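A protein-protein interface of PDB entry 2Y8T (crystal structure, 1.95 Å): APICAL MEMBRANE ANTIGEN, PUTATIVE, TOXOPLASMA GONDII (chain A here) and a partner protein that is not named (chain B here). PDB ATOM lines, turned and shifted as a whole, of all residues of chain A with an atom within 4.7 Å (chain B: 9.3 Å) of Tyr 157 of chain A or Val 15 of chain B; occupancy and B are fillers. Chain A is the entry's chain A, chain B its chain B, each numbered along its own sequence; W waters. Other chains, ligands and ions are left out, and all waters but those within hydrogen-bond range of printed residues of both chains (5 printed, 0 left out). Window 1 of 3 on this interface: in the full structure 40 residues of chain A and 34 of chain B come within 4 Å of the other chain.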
ATOM      1  N   PHE A 105      25.028  24.276  13.550  1.00  0.00           N
ATOM      2  CA  PHE A 105      25.138  25.431  12.657  1.00  0.00           C
ATOM      3  C   PHE A 105      26.495  25.431  11.921  1.00  0.00           C
ATOM      4  O   PHE A 105      27.491  24.897  12.416  1.00  0.00           O
ATOM      5  CB  PHE A 105      25.014  26.725  13.447  1.00  0.00           C
ATOM      6  CG  PHE A 105      23.629  26.964  14.061  1.00  0.00           C
ATOM      7  CD1 PHE A 105      22.608  26.025  13.956  1.00  0.00           C
ATOM      8  CD2 PHE A 105      23.428  28.083  14.862  1.00  0.00           C
ATOM      9  CE1 PHE A 105      21.309  26.263  14.527  1.00  0.00           C
ATOM     10  CE2 PHE A 105      22.170  28.297  15.496  1.00  0.00           C
ATOM     11  CZ  PHE A 105      21.112  27.353  15.312  1.00  0.00           C
ATOM     12  N   ALA A 140      33.187  27.883  24.054  1.00  0.00           N
ATOM     13  CA  ALA A 140      31.753  28.017  24.422  1.00  0.00           C
ATOM     14  C   ALA A 140      31.424  29.452  24.904  1.00  0.00           C
ATOM     15  O   ALA A 140      30.369  30.024  24.524  1.00  0.00           O
ATOM     16  CB  ALA A 140      31.360  26.978  25.486  1.00  0.00           C
ATOM     17  N   ALA A 145      24.167  33.528  21.307  1.00  0.00           N
ATOM     18  CA  ALA A 145      22.966  33.459  20.449  1.00  0.00           C
ATOM     19  C   ALA A 145      22.754  34.828  19.797  1.00  0.00           C
ATOM     20  O   ALA A 145      22.970  35.859  20.420  1.00  0.00           O
ATOM     21  CB  ALA A 145      21.726  33.082  21.326  1.00  0.00           C
ATOM     22  N   MET A 146      22.337  34.842  18.537  1.00  0.00           N
ATOM     23  CA  MET A 146      21.847  36.042  17.887  1.00  0.00           C
ATOM     24  C   MET A 146      20.308  36.035  17.903  1.00  0.00           C
ATOM     25  O   MET A 146      19.657  34.995  17.731  1.00  0.00           O
ATOM     26  CB  MET A 146      22.375  36.104  16.438  1.00  0.00           C
ATOM     27  CG  MET A 146      23.937  36.304  16.430  1.00  0.00           C
ATOM     28  SD  MET A 146      24.669  35.736  14.905  1.00  0.00           S
ATOM     29  CE  MET A 146      23.751  36.802  13.737  1.00  0.00           C
ATOM     30  N   TYR A 155      23.122  35.548  25.717  1.00  0.00           N
ATOM     31  CA  TYR A 155      22.695  34.183  26.070  1.00  0.00           C
ATOM     32  C   TYR A 155      23.747  33.243  25.460  1.00  0.00           C
ATOM     33  O   TYR A 155      24.069  33.340  24.249  1.00  0.00           O
ATOM     34  CB  TYR A 155      21.310  33.893  25.476  1.00  0.00           C
ATOM     35  CG  TYR A 155      20.841  32.479  25.766  1.00  0.00           C
ATOM     36  CD1 TYR A 155      21.296  31.388  24.984  1.00  0.00           C
ATOM     37  CD2 TYR A 155      19.953  32.225  26.807  1.00  0.00           C
ATOM     38  CE1 TYR A 155      20.900  30.070  25.247  1.00  0.00           C
ATOM     39  CE2 TYR A 155      19.489  30.882  27.052  1.00  0.00           C
ATOM     40  CZ  TYR A 155      19.953  29.841  26.249  1.00  0.00           C
ATOM     41  OH  TYR A 155      19.602  28.550  26.480  1.00  0.00           O
ATOM     42  N   ARG A 156      24.199  32.270  26.260  1.00  0.00           N
ATOM     43  CA  ARG A 156      25.236  31.290  25.870  1.00  0.00           C
ATOM     44  C   ARG A 156      24.786  29.865  26.137  1.00  0.00           C
ATOM     45  O   ARG A 156      24.299  29.561  27.230  1.00  0.00           O
ATOM     46  CB  ARG A 156      26.526  31.544  26.631  1.00  0.00           C
ATOM     47  CG  ARG A 156      27.163  32.894  26.222  1.00  0.00           C
ATOM     48  CD  ARG A 156      28.406  33.192  27.091  1.00  0.00           C
ATOM     49  NE  ARG A 156      29.078  34.447  26.727  1.00  0.00           N
ATOM     50  CZ  ARG A 156      28.712  35.680  27.066  1.00  0.00           C
ATOM     51  NH1 ARG A 156      27.691  35.917  27.894  1.00  0.00           N
ATOM     52  NH2 ARG A 156      29.460  36.696  26.633  1.00  0.00           N
ATOM     53  N   TYR A 157      24.889  29.015  25.124  1.00  0.00           N
ATOM     54  CA  TYR A 157      24.612  27.593  25.295  1.00  0.00           C
ATOM     55  C   TYR A 157      25.702  26.865  26.104  1.00  0.00           C
ATOM     56  O   TYR A 157      26.868  27.270  26.029  1.00  0.00           O
ATOM     57  CB  TYR A 157      24.573  27.025  23.918  1.00  0.00           C
ATOM     58  CG  TYR A 157      23.426  27.592  23.150  1.00  0.00           C
ATOM     59  CD1 TYR A 157      22.180  27.055  23.292  1.00  0.00           C
ATOM     60  CD2 TYR A 157      23.601  28.680  22.286  1.00  0.00           C
ATOM     61  CE1 TYR A 157      21.081  27.591  22.550  1.00  0.00           C
ATOM     62  CE2 TYR A 157      22.545  29.220  21.564  1.00  0.00           C
ATOM     63  CZ  TYR A 157      21.305  28.669  21.677  1.00  0.00           C
ATOM     64  OH  TYR A 157      20.254  29.223  20.947  1.00  0.00           O
ATOM     65  N   PRO A 158      25.333  25.767  26.822  1.00  0.00           N
ATOM     66  CA  PRO A 158      26.297  24.949  27.530  1.00  0.00           C
ATOM     67  C   PRO A 158      27.105  24.098  26.547  1.00  0.00           C
ATOM     68  O   PRO A 158      26.783  24.031  25.348  1.00  0.00           O
ATOM     69  CB  PRO A 158      25.426  24.063  28.431  1.00  0.00           C
ATOM     70  CG  PRO A 158      24.099  23.870  27.606  1.00  0.00           C
ATOM     71  CD  PRO A 158      23.937  25.259  26.986  1.00  0.00           C
ATOM     72  N   PHE A 159      28.180  23.498  27.057  1.00  0.00           N
ATOM     73  CA  PHE A 159      29.081  22.694  26.257  1.00  0.00           C
ATOM     74  C   PHE A 159      29.306  21.342  26.867  1.00  0.00           C
ATOM     75  O   PHE A 159      29.058  21.124  28.054  1.00  0.00           O
ATOM     76  CB  PHE A 159      30.450  23.401  26.031  1.00  0.00           C
ATOM     77  CG  PHE A 159      31.330  23.411  27.259  1.00  0.00           C
ATOM     78  CD1 PHE A 159      31.164  24.373  28.248  1.00  0.00           C
ATOM     79  CD2 PHE A 159      32.257  22.386  27.459  1.00  0.00           C
ATOM     80  CE1 PHE A 159      31.947  24.356  29.446  1.00  0.00           C
ATOM     81  CE2 PHE A 159      33.041  22.341  28.631  1.00  0.00           C
ATOM     82  CZ  PHE A 159      32.931  23.353  29.623  1.00  0.00           C
ATOM     83  N   ILE A 170      28.998  22.252  21.472  1.00  0.00           N
ATOM     84  CA  ILE A 170      28.071  23.239  21.982  1.00  0.00           C
ATOM     85  C   ILE A 170      26.665  22.640  21.863  1.00  0.00           C
ATOM     86  O   ILE A 170      26.312  22.095  20.815  1.00  0.00           O
ATOM     87  CB  ILE A 170      28.145  24.522  21.144  1.00  0.00           C
ATOM     88  CG1 ILE A 170      29.588  25.131  21.176  1.00  0.00           C
ATOM     89  CG2 ILE A 170      27.123  25.587  21.650  1.00  0.00           C
ATOM     90  CD1 ILE A 170      30.191  25.302  22.596  1.00  0.00           C
ATOM     91  N   LEU A 171      25.869  22.721  22.915  1.00  0.00           N
ATOM     92  CA  LEU A 171      24.507  22.132  22.873  1.00  0.00           C
ATOM     93  C   LEU A 171      23.492  23.198  22.598  1.00  0.00           C
ATOM     94  O   LEU A 171      23.385  24.133  23.368  1.00  0.00           O
ATOM     95  CB  LEU A 171      24.142  21.526  24.208  1.00  0.00           C
ATOM     96  CG  LEU A 171      25.074  20.445  24.768  1.00  0.00           C
ATOM     97  CD1 LEU A 171      24.452  19.788  26.050  1.00  0.00           C
ATOM     98  CD2 LEU A 171      25.349  19.379  23.709  1.00  0.00           C
ATOM     99  N   TYR A 172      22.700  23.039  21.536  1.00  0.00           N
ATOM    100  CA  TYR A 172      21.573  23.945  21.278  1.00  0.00           C
ATOM    101  C   TYR A 172      20.449  23.780  22.326  1.00  0.00           C
ATOM    102  O   TYR A 172      19.571  24.633  22.476  1.00  0.00           O
ATOM    103  CB  TYR A 172      21.057  23.595  19.892  1.00  0.00           C
ATOM    104  CG  TYR A 172      20.014  24.508  19.266  1.00  0.00           C
ATOM    105  CD1 TYR A 172      20.275  25.853  19.012  1.00  0.00           C
ATOM    106  CD2 TYR A 172      18.764  24.002  18.919  1.00  0.00           C
ATOM    107  CE1 TYR A 172      19.300  26.682  18.368  1.00  0.00           C
ATOM    108  CE2 TYR A 172      17.796  24.813  18.318  1.00  0.00           C
ATOM    109  CZ  TYR A 172      18.092  26.146  18.012  1.00  0.00           C
ATOM    110  OH  TYR A 172      17.103  26.932  17.428  1.00  0.00           O
ATOM    111  N   SER A 174      19.577  23.547  26.057  1.00  0.00           N
ATOM    112  CA  SER A 174      20.015  23.819  27.406  1.00  0.00           C
ATOM    113  C   SER A 174      19.138  23.112  28.470  1.00  0.00           C
ATOM    114  O   SER A 174      19.547  23.028  29.614  1.00  0.00           O
ATOM    115  CB  SER A 174      19.942  25.333  27.642  1.00  0.00           C
ATOM    116  OG  SER A 174      20.823  25.957  26.740  1.00  0.00           O
ATOM    117  N   ALA A 215      28.567  27.665  29.627  1.00  0.00           N
ATOM    118  CA  ALA A 215      29.594  28.401  28.848  1.00  0.00           C
ATOM    119  C   ALA A 215      30.421  29.242  29.804  1.00  0.00           C
ATOM    120  O   ALA A 215      31.512  29.692  29.431  1.00  0.00           O
ATOM    121  CB  ALA A 215      28.940  29.338  27.827  1.00  0.00           C
ATOM    122  N   GLY B  10      14.261  25.225  31.036  1.00  0.00           N
ATOM    123  CA  GLY B  10      15.438  25.566  30.258  1.00  0.00           C
ATOM    124  C   GLY B  10      15.208  25.605  28.740  1.00  0.00           C
ATOM    125  O   GLY B  10      16.157  25.659  27.970  1.00  0.00           O
ATOM    126  N   GLY B  11      13.964  25.573  28.297  1.00  0.00           N
ATOM    127  CA  GLY B  11      13.633  25.687  26.839  1.00  0.00           C
ATOM    128  C   GLY B  11      14.316  26.950  26.267  1.00  0.00           C
ATOM    129  O   GLY B  11      14.235  27.999  26.847  1.00  0.00           O
ATOM    130  N   ALA B  12      15.062  26.832  25.168  1.00  0.00           N
ATOM    131  CA  ALA B  12      15.922  27.937  24.722  1.00  0.00           C
ATOM    132  C   ALA B  12      15.275  28.861  23.653  1.00  0.00           C
ATOM    133  O   ALA B  12      14.259  28.533  23.078  1.00  0.00           O
ATOM    134  CB  ALA B  12      17.266  27.375  24.246  1.00  0.00           C
ATOM    135  N   PRO B  13      15.770  30.097  23.497  1.00  0.00           N
ATOM    136  CA  PRO B  13      15.132  30.944  22.481  1.00  0.00           C
ATOM    137  C   PRO B  13      15.092  30.301  21.068  1.00  0.00           C
ATOM    138  O   PRO B  13      15.935  29.477  20.715  1.00  0.00           O
ATOM    139  CB  PRO B  13      15.994  32.232  22.463  1.00  0.00           C
ATOM    140  CG  PRO B  13      17.255  31.922  23.268  1.00  0.00           C
ATOM    141  CD  PRO B  13      17.007  30.663  24.085  1.00  0.00           C
ATOM    142  N   PRO B  14      14.103  30.673  20.256  1.00  0.00           N
ATOM    143  CA  PRO B  14      14.106  30.186  18.863  1.00  0.00           C
ATOM    144  C   PRO B  14      15.177  30.927  18.024  1.00  0.00           C
ATOM    145  O   PRO B  14      14.944  32.037  17.526  1.00  0.00           O
ATOM    146  CB  PRO B  14      12.666  30.454  18.381  1.00  0.00           C
ATOM    147  CG  PRO B  14      12.124  31.478  19.285  1.00  0.00           C
ATOM    148  CD  PRO B  14      12.849  31.345  20.623  1.00  0.00           C
ATOM    149  N   VAL B  15      16.371  30.352  17.972  1.00  0.00           N
ATOM    150  CA  VAL B  15      17.537  31.033  17.470  1.00  0.00           C
ATOM    151  C   VAL B  15      17.913  30.266  16.195  1.00  0.00           C
ATOM    152  O   VAL B  15      17.913  29.032  16.199  1.00  0.00           O
ATOM    153  CB  VAL B  15      18.686  30.956  18.540  1.00  0.00           C
ATOM    154  CG1 VAL B  15      20.075  31.152  17.924  1.00  0.00           C
ATOM    155  CG2 VAL B  15      18.411  31.958  19.688  1.00  0.00           C
ATOM    156  N   SER B  16      18.238  30.991  15.119  1.00  0.00           N
ATOM    157  CA  SER B  16      18.750  30.350  13.870  1.00  0.00           C
ATOM    158  C   SER B  16      20.261  30.528  13.680  1.00  0.00           C
ATOM    159  O   SER B  16      20.835  29.905  12.796  1.00  0.00           O
ATOM    160  CB  SER B  16      18.089  30.982  12.623  1.00  0.00           C
ATOM    161  OG  SER B  16      16.892  30.311  12.440  1.00  0.00           O
ATOM    162  N   CYS B  17      20.865  31.433  14.436  1.00  0.00           N
ATOM    163  CA  CYS B  17      22.291  31.809  14.214  1.00  0.00           C
ATOM    164  C   CYS B  17      22.975  32.062  15.560  1.00  0.00           C
ATOM    165  O   CYS B  17      22.361  32.577  16.481  1.00  0.00           O
ATOM    166  CB  CYS B  17      22.424  33.112  13.371  1.00  0.00           C
ATOM    167  SG  CYS B  17      21.828  32.896  11.638  1.00  0.00           S
ATOM    168  N   VAL B  18      24.269  31.761  15.612  1.00  0.00           N
ATOM    169  CA  VAL B  18      25.069  32.094  16.746  1.00  0.00           C
ATOM    170  C   VAL B  18      26.313  32.833  16.234  1.00  0.00           C
ATOM    171  O   VAL B  18      26.686  32.616  15.111  1.00  0.00           O
ATOM    172  CB  VAL B  18      25.354  30.712  17.318  1.00  0.00           C
ATOM    173  CG1 VAL B  18      26.749  30.294  17.397  1.00  0.00           C
ATOM    174  CG2 VAL B  18      24.288  30.272  18.342  1.00  0.00           C
ATOM    175  N   THR B  19      26.888  33.766  16.988  1.00  0.00           N
ATOM    176  CA  THR B  19      28.218  34.285  16.607  1.00  0.00           C
ATOM    177  C   THR B  19      29.318  33.817  17.554  1.00  0.00           C
ATOM    178  O   THR B  19      29.181  33.935  18.783  1.00  0.00           O
ATOM    179  CB  THR B  19      28.281  35.800  16.408  1.00  0.00           C
ATOM    180  OG1 THR B  19      29.580  36.179  15.895  1.00  0.00           O
ATOM    181  CG2 THR B  19      27.917  36.623  17.688  1.00  0.00           C
ATOM    182  N   THR B  26      27.361  31.840  12.395  1.00  0.00           N
ATOM    183  CA  THR B  26      27.180  30.476  12.002  1.00  0.00           C
ATOM    184  C   THR B  26      25.631  30.239  12.095  1.00  0.00           C
ATOM    185  O   THR B  26      24.978  30.740  13.014  1.00  0.00           O
ATOM    186  CB  THR B  26      28.027  29.696  13.030  1.00  0.00           C
ATOM    187  OG1 THR B  26      29.234  29.089  12.534  1.00  0.00           O
ATOM    188  CG2 THR B  26      27.333  29.083  14.137  1.00  0.00           C
ATOM    189  N   CYS B  27      25.052  29.553  11.125  1.00  0.00           N
ATOM    190  CA  CYS B  27      23.582  29.483  11.034  1.00  0.00           C
ATOM    191  C   CYS B  27      23.180  28.074  10.696  1.00  0.00           C
ATOM    192  O   CYS B  27      23.939  27.360  10.154  1.00  0.00           O
ATOM    193  CB  CYS B  27      23.053  30.449   9.957  1.00  0.00           C
ATOM    194  SG  CYS B  27      23.357  32.205  10.310  1.00  0.00           S
ATOM    195  N   ALA B  28      21.950  27.691  11.007  1.00  0.00           N
ATOM    196  CA  ALA B  28      21.429  26.416  10.559  1.00  0.00           C
ATOM    197  C   ALA B  28      21.333  26.396   9.025  1.00  0.00           C
ATOM    198  O   ALA B  28      20.621  27.237   8.467  1.00  0.00           O
ATOM    199  CB  ALA B  28      20.060  26.244  11.135  1.00  0.00           C
ATOM    200  N   GLN B  30      19.592  24.270   7.285  1.00  0.00           N
ATOM    201  CA  GLN B  30      18.186  23.820   6.985  1.00  0.00           C
ATOM    202  C   GLN B  30      17.316  24.093   8.187  1.00  0.00           C
ATOM    203  O   GLN B  30      17.839  24.191   9.306  1.00  0.00           O
ATOM    204  CB  GLN B  30      18.085  22.313   6.743  1.00  0.00           C
ATOM    205  CG  GLN B  30      19.143  21.727   5.854  1.00  0.00           C
ATOM    206  CD  GLN B  30      18.863  20.261   5.578  1.00  0.00           C
ATOM    207  OE1 GLN B  30      17.930  19.907   4.838  1.00  0.00           O
ATOM    208  NE2 GLN B  30      19.637  19.398   6.209  1.00  0.00           N
ATOM    209  N   ALA B  31      16.000  24.196   7.986  1.00  0.00           N
ATOM    210  CA  ALA B  31      15.111  24.544   9.102  1.00  0.00           C
ATOM    211  C   ALA B  31      15.229  23.488  10.204  1.00  0.00           C
ATOM    212  O   ALA B  31      15.203  22.290   9.925  1.00  0.00           O
ATOM    213  CB  ALA B  31      13.663  24.686   8.655  1.00  0.00           C
ATOM    214  N   ILE B  32      15.395  23.947  11.434  1.00  0.00           N
ATOM    215  CA  ILE B  32      15.500  23.035  12.587  1.00  0.00           C
ATOM    216  C   ILE B  32      14.058  22.646  12.933  1.00  0.00           C
ATOM    217  O   ILE B  32      13.161  23.457  12.778  1.00  0.00           O
ATOM    218  CB  ILE B  32      16.130  23.770  13.814  1.00  0.00           C
ATOM    219  CG1 ILE B  32      17.591  24.194  13.529  1.00  0.00           C
ATOM    220  CG2 ILE B  32      16.193  22.849  15.044  1.00  0.00           C
ATOM    221  CD1 ILE B  32      18.459  22.987  13.118  1.00  0.00           C
ATOM    222  N   ALA B  33      13.816  21.422  13.364  1.00  0.00           N
ATOM    223  CA  ALA B  33      12.477  21.068  13.858  1.00  0.00           C
ATOM    224  C   ALA B  33      11.932  22.148  14.821  1.00  0.00           C
ATOM    225  O   ALA B  33      12.630  22.645  15.747  1.00  0.00           O
ATOM    226  CB  ALA B  33      12.497  19.704  14.518  1.00  0.00           C
ATOM    227  N   LYS B  34      10.671  22.508  14.599  1.00  0.00           N
ATOM    228  CA  LYS B  34      10.056  23.644  15.281  1.00  0.00           C
ATOM    229  C   LYS B  34      10.024  23.423  16.798  1.00  0.00           C
ATOM    230  O   LYS B  34      10.390  24.304  17.596  1.00  0.00           O
ATOM    231  CB  LYS B  34       8.641  23.884  14.717  1.00  0.00           C
ATOM    232  CG  LYS B  34       8.632  24.362  13.249  1.00  0.00           C
ATOM    233  CD  LYS B  34       9.391  25.723  13.107  1.00  0.00           C
ATOM    234  CE  LYS B  34       9.759  26.071  11.641  1.00  0.00           C
ATOM    235  NZ  LYS B  34      10.636  25.039  10.993  1.00  0.00           N
ATOM    236  N   THR B  36      11.930  21.861  18.738  1.00  0.00           N
ATOM    237  CA  THR B  36      13.242  21.746  19.404  1.00  0.00           C
ATOM    238  C   THR B  36      13.699  22.994  20.185  1.00  0.00           C
ATOM    239  O   THR B  36      13.359  23.186  21.367  1.00  0.00           O
ATOM    240  CB  THR B  36      14.357  21.356  18.409  1.00  0.00           C
ATOM    241  OG1 THR B  36      14.123  20.016  17.937  1.00  0.00           O
ATOM    242  CG2 THR B  36      15.731  21.414  19.097  1.00  0.00           C
ATOM    243  N   9AT B  37      13.136  24.384  19.126  1.00  0.00           N
ATOM    244  CA  9AT B  37      12.689  25.767  18.874  1.00  0.00           C
ATOM    245  C   9AT B  37      13.124  26.177  17.451  1.00  0.00           C
ATOM    246  O   9AT B  37      14.306  26.224  17.093  1.00  0.00           O
ATOM    247  CB  9AT B  37      13.201  26.654  19.991  1.00  0.00           C
ATOM    248  OG1 9AT B  37      14.578  26.367  20.118  1.00  0.00           O
ATOM    249  CG2 9AT B  37      12.497  26.261  21.287  1.00  0.00           C
ATOM    250  NXT 9AT B  37      12.124  26.182  16.586  1.00  0.00           N
HETATM  251  O   HOH W   1      17.920  28.179  21.084  1.00  0.00           O
HETATM  252  O   HOH W   2      17.355  28.293  27.648  1.00  0.00           O
HETATM  253  O   HOH W   3      16.799  24.171  25.782  1.00  0.00           O
HETATM  254  O   HOH W   4      19.114  33.715  15.384  1.00  0.00           O
HETATM  255  O   HOH W   5      17.183  25.318  21.567  1.00  0.00           O
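The backbone carbonyl oxygen (O) of Cys 17 of chain B sits at hydrogen-bond distance from the backbone NH (N) of Met 146 of chain A (3.1 Å).
N of Thr 19 of chain B sits at hydrogen-bond distance from SD of Met 146 of chain A.
O of Val 15 of chain B lies within hydrogen-bond range of OH of Tyr 172 of chain A (2.6 Å).
OH of Tyr 172 of chain A sits at hydrogen-bond distance from O of 9AT 37 of chain B (2.9 Å).
The side-chain sulfur of Met 146 of chain A sits close to the backbone carbonyl oxygen of Val 18 of chain B, 3.7 Å away.
Hydrophobic or aromatic side chains of chain A within 4 Å of the printed part of chain B: Phe 105, Ala 145, Met 146, Tyr 155, Tyr 157 and Tyr 172.
Of the 20 printed residues of chain B, 13 touch a printed residue of chain A.
Hydrophobic or aromatic side chains of chain B that line the printed part of chain A: Ala 12, Pro 13, Val 15, Val 18 and Ala 28.
Along chain B the printed residues that touch a printed residue of chain A span positions 10 to 37.
Among the printed residues, no Asp or Glu carboxylate lies within 4 Å of a Lys or Arg side-chain nitrogen of the other chain.
Phe 105 of chain A touches Val 18 of chain B (CD2 to N, 3.8 Å).
Phe 105 of chain A touches Thr 26 of chain B.
Cys 27 of chain B touches Phe 105 of chain A (O to CA, 3.4 Å).
Val 15 of chain B touches Ala 145 of chain A (CG2 to CB, 3.9 Å).
Tyr 155 of chain A touches Ala 12 of chain B (OH to CB, 3.4 Å).
Pro 13 of chain B touches Tyr 155 of chain A (CD to CZ, 3.7 Å).
Tyr 157 of chain A touches Val 15 of chain B.
Val 18 of chain B touches Tyr 157 of chain A (CG2 to CE2, 3.8 Å).
Tyr 172 of chain A touches Ala 12 of chain B.
Gly 10 of chain B touches Ser 174 of chain A (O to CB, 3.8 Å).
Water W1 lies within hydrogen-bond range of the backbone carbonyl oxygen of Pro 13 of chain B (2.4 Å) and the side-chain hydroxyl of Tyr 157 of chain A (2.6 Å).
Water W2 lies within hydrogen-bond range of OH of Tyr 155 of chain A (2.5 Å), O of Gly 10 of chain B (2.9 Å) and O of Gly 11 of chain B (3.2 Å).
Water W5 lies within hydrogen-bond range of the backbone carbonyl oxygen of Tyr 172 of chain A (2.6 Å) and OG1 of 9AT 37 of chain B (3.2 Å).
Water W3 lies within hydrogen-bond range of the backbone carbonyl oxygen (O) of Gly 10 of chain B (2.7 Å), the backbone NH (N) of Ser 174 of chain A (2.9 Å) and the backbone NH (N) of Ala 12 of chain B (3.2 Å).
Water W4 lies within hydrogen-bond range of the backbone carbonyl oxygen of Met 146 of chain A (2.7 Å), the backbone NH of Ser 16 of chain B (2.9 Å) and the backbone NH of Cys 17 of chain B (3.0 Å).
Tyr 157 of chain A touches just these residues of chain B: Val 15 (3.4 Å) and Val 18 (3.8 Å).
Ile 170 of chain A touches none of the printed residues of chain B.
Printed residues of chain B within 4 Å of Ser 174 of chain A: Gly 10 (3.8 Å).
Val 15 of chain B touches just these residues of chain A: Phe 105 (3.7 Å), Ala 145 (3.9 Å), Met 146 (3.8 Å), Tyr 157 (3.4 Å) and Tyr 172 (2.6 Å).
Of the printed residues of chain A, 9AT 37 of chain B touches Tyr 172 (2.9 Å).
The nearest residue of chain B that does not touch Tyr 157 of chain A is Ala 12 of chain B (4.2 Å).
The nearest printed residue of chain A that does not touch Val 15 of chain B is Tyr 155 of chain A (6.1 Å).
The backbone NH of Ala 145 of chain A is in hydrogen-bond range of the backbone carbonyl oxygen of Tyr 155 of chain A (2.9 Å).
OG of Ser 174 of chain A sits at hydrogen-bond distance from OH of Tyr 155 of chain A (2.9 Å).
The backbone carbonyl oxygen (O) of Pro 13 of chain B is in hydrogen-bond range of OG1 of 9AT 37 of chain B, 3.4 Å away.
O of Ser 16 of chain B lies within hydrogen-bond range of N of Ala 28 of chain B, 3.1 Å away.
The side-chain sulfur of Cys 17 of chain B is disulfide-bonded to the side-chain sulfur of Cys 27 of chain B (2.1 Å).
The backbone NH (N) of Val 18 of chain B sits at hydrogen-bond distance from the backbone carbonyl oxygen (O) of Thr 26 of chain B.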
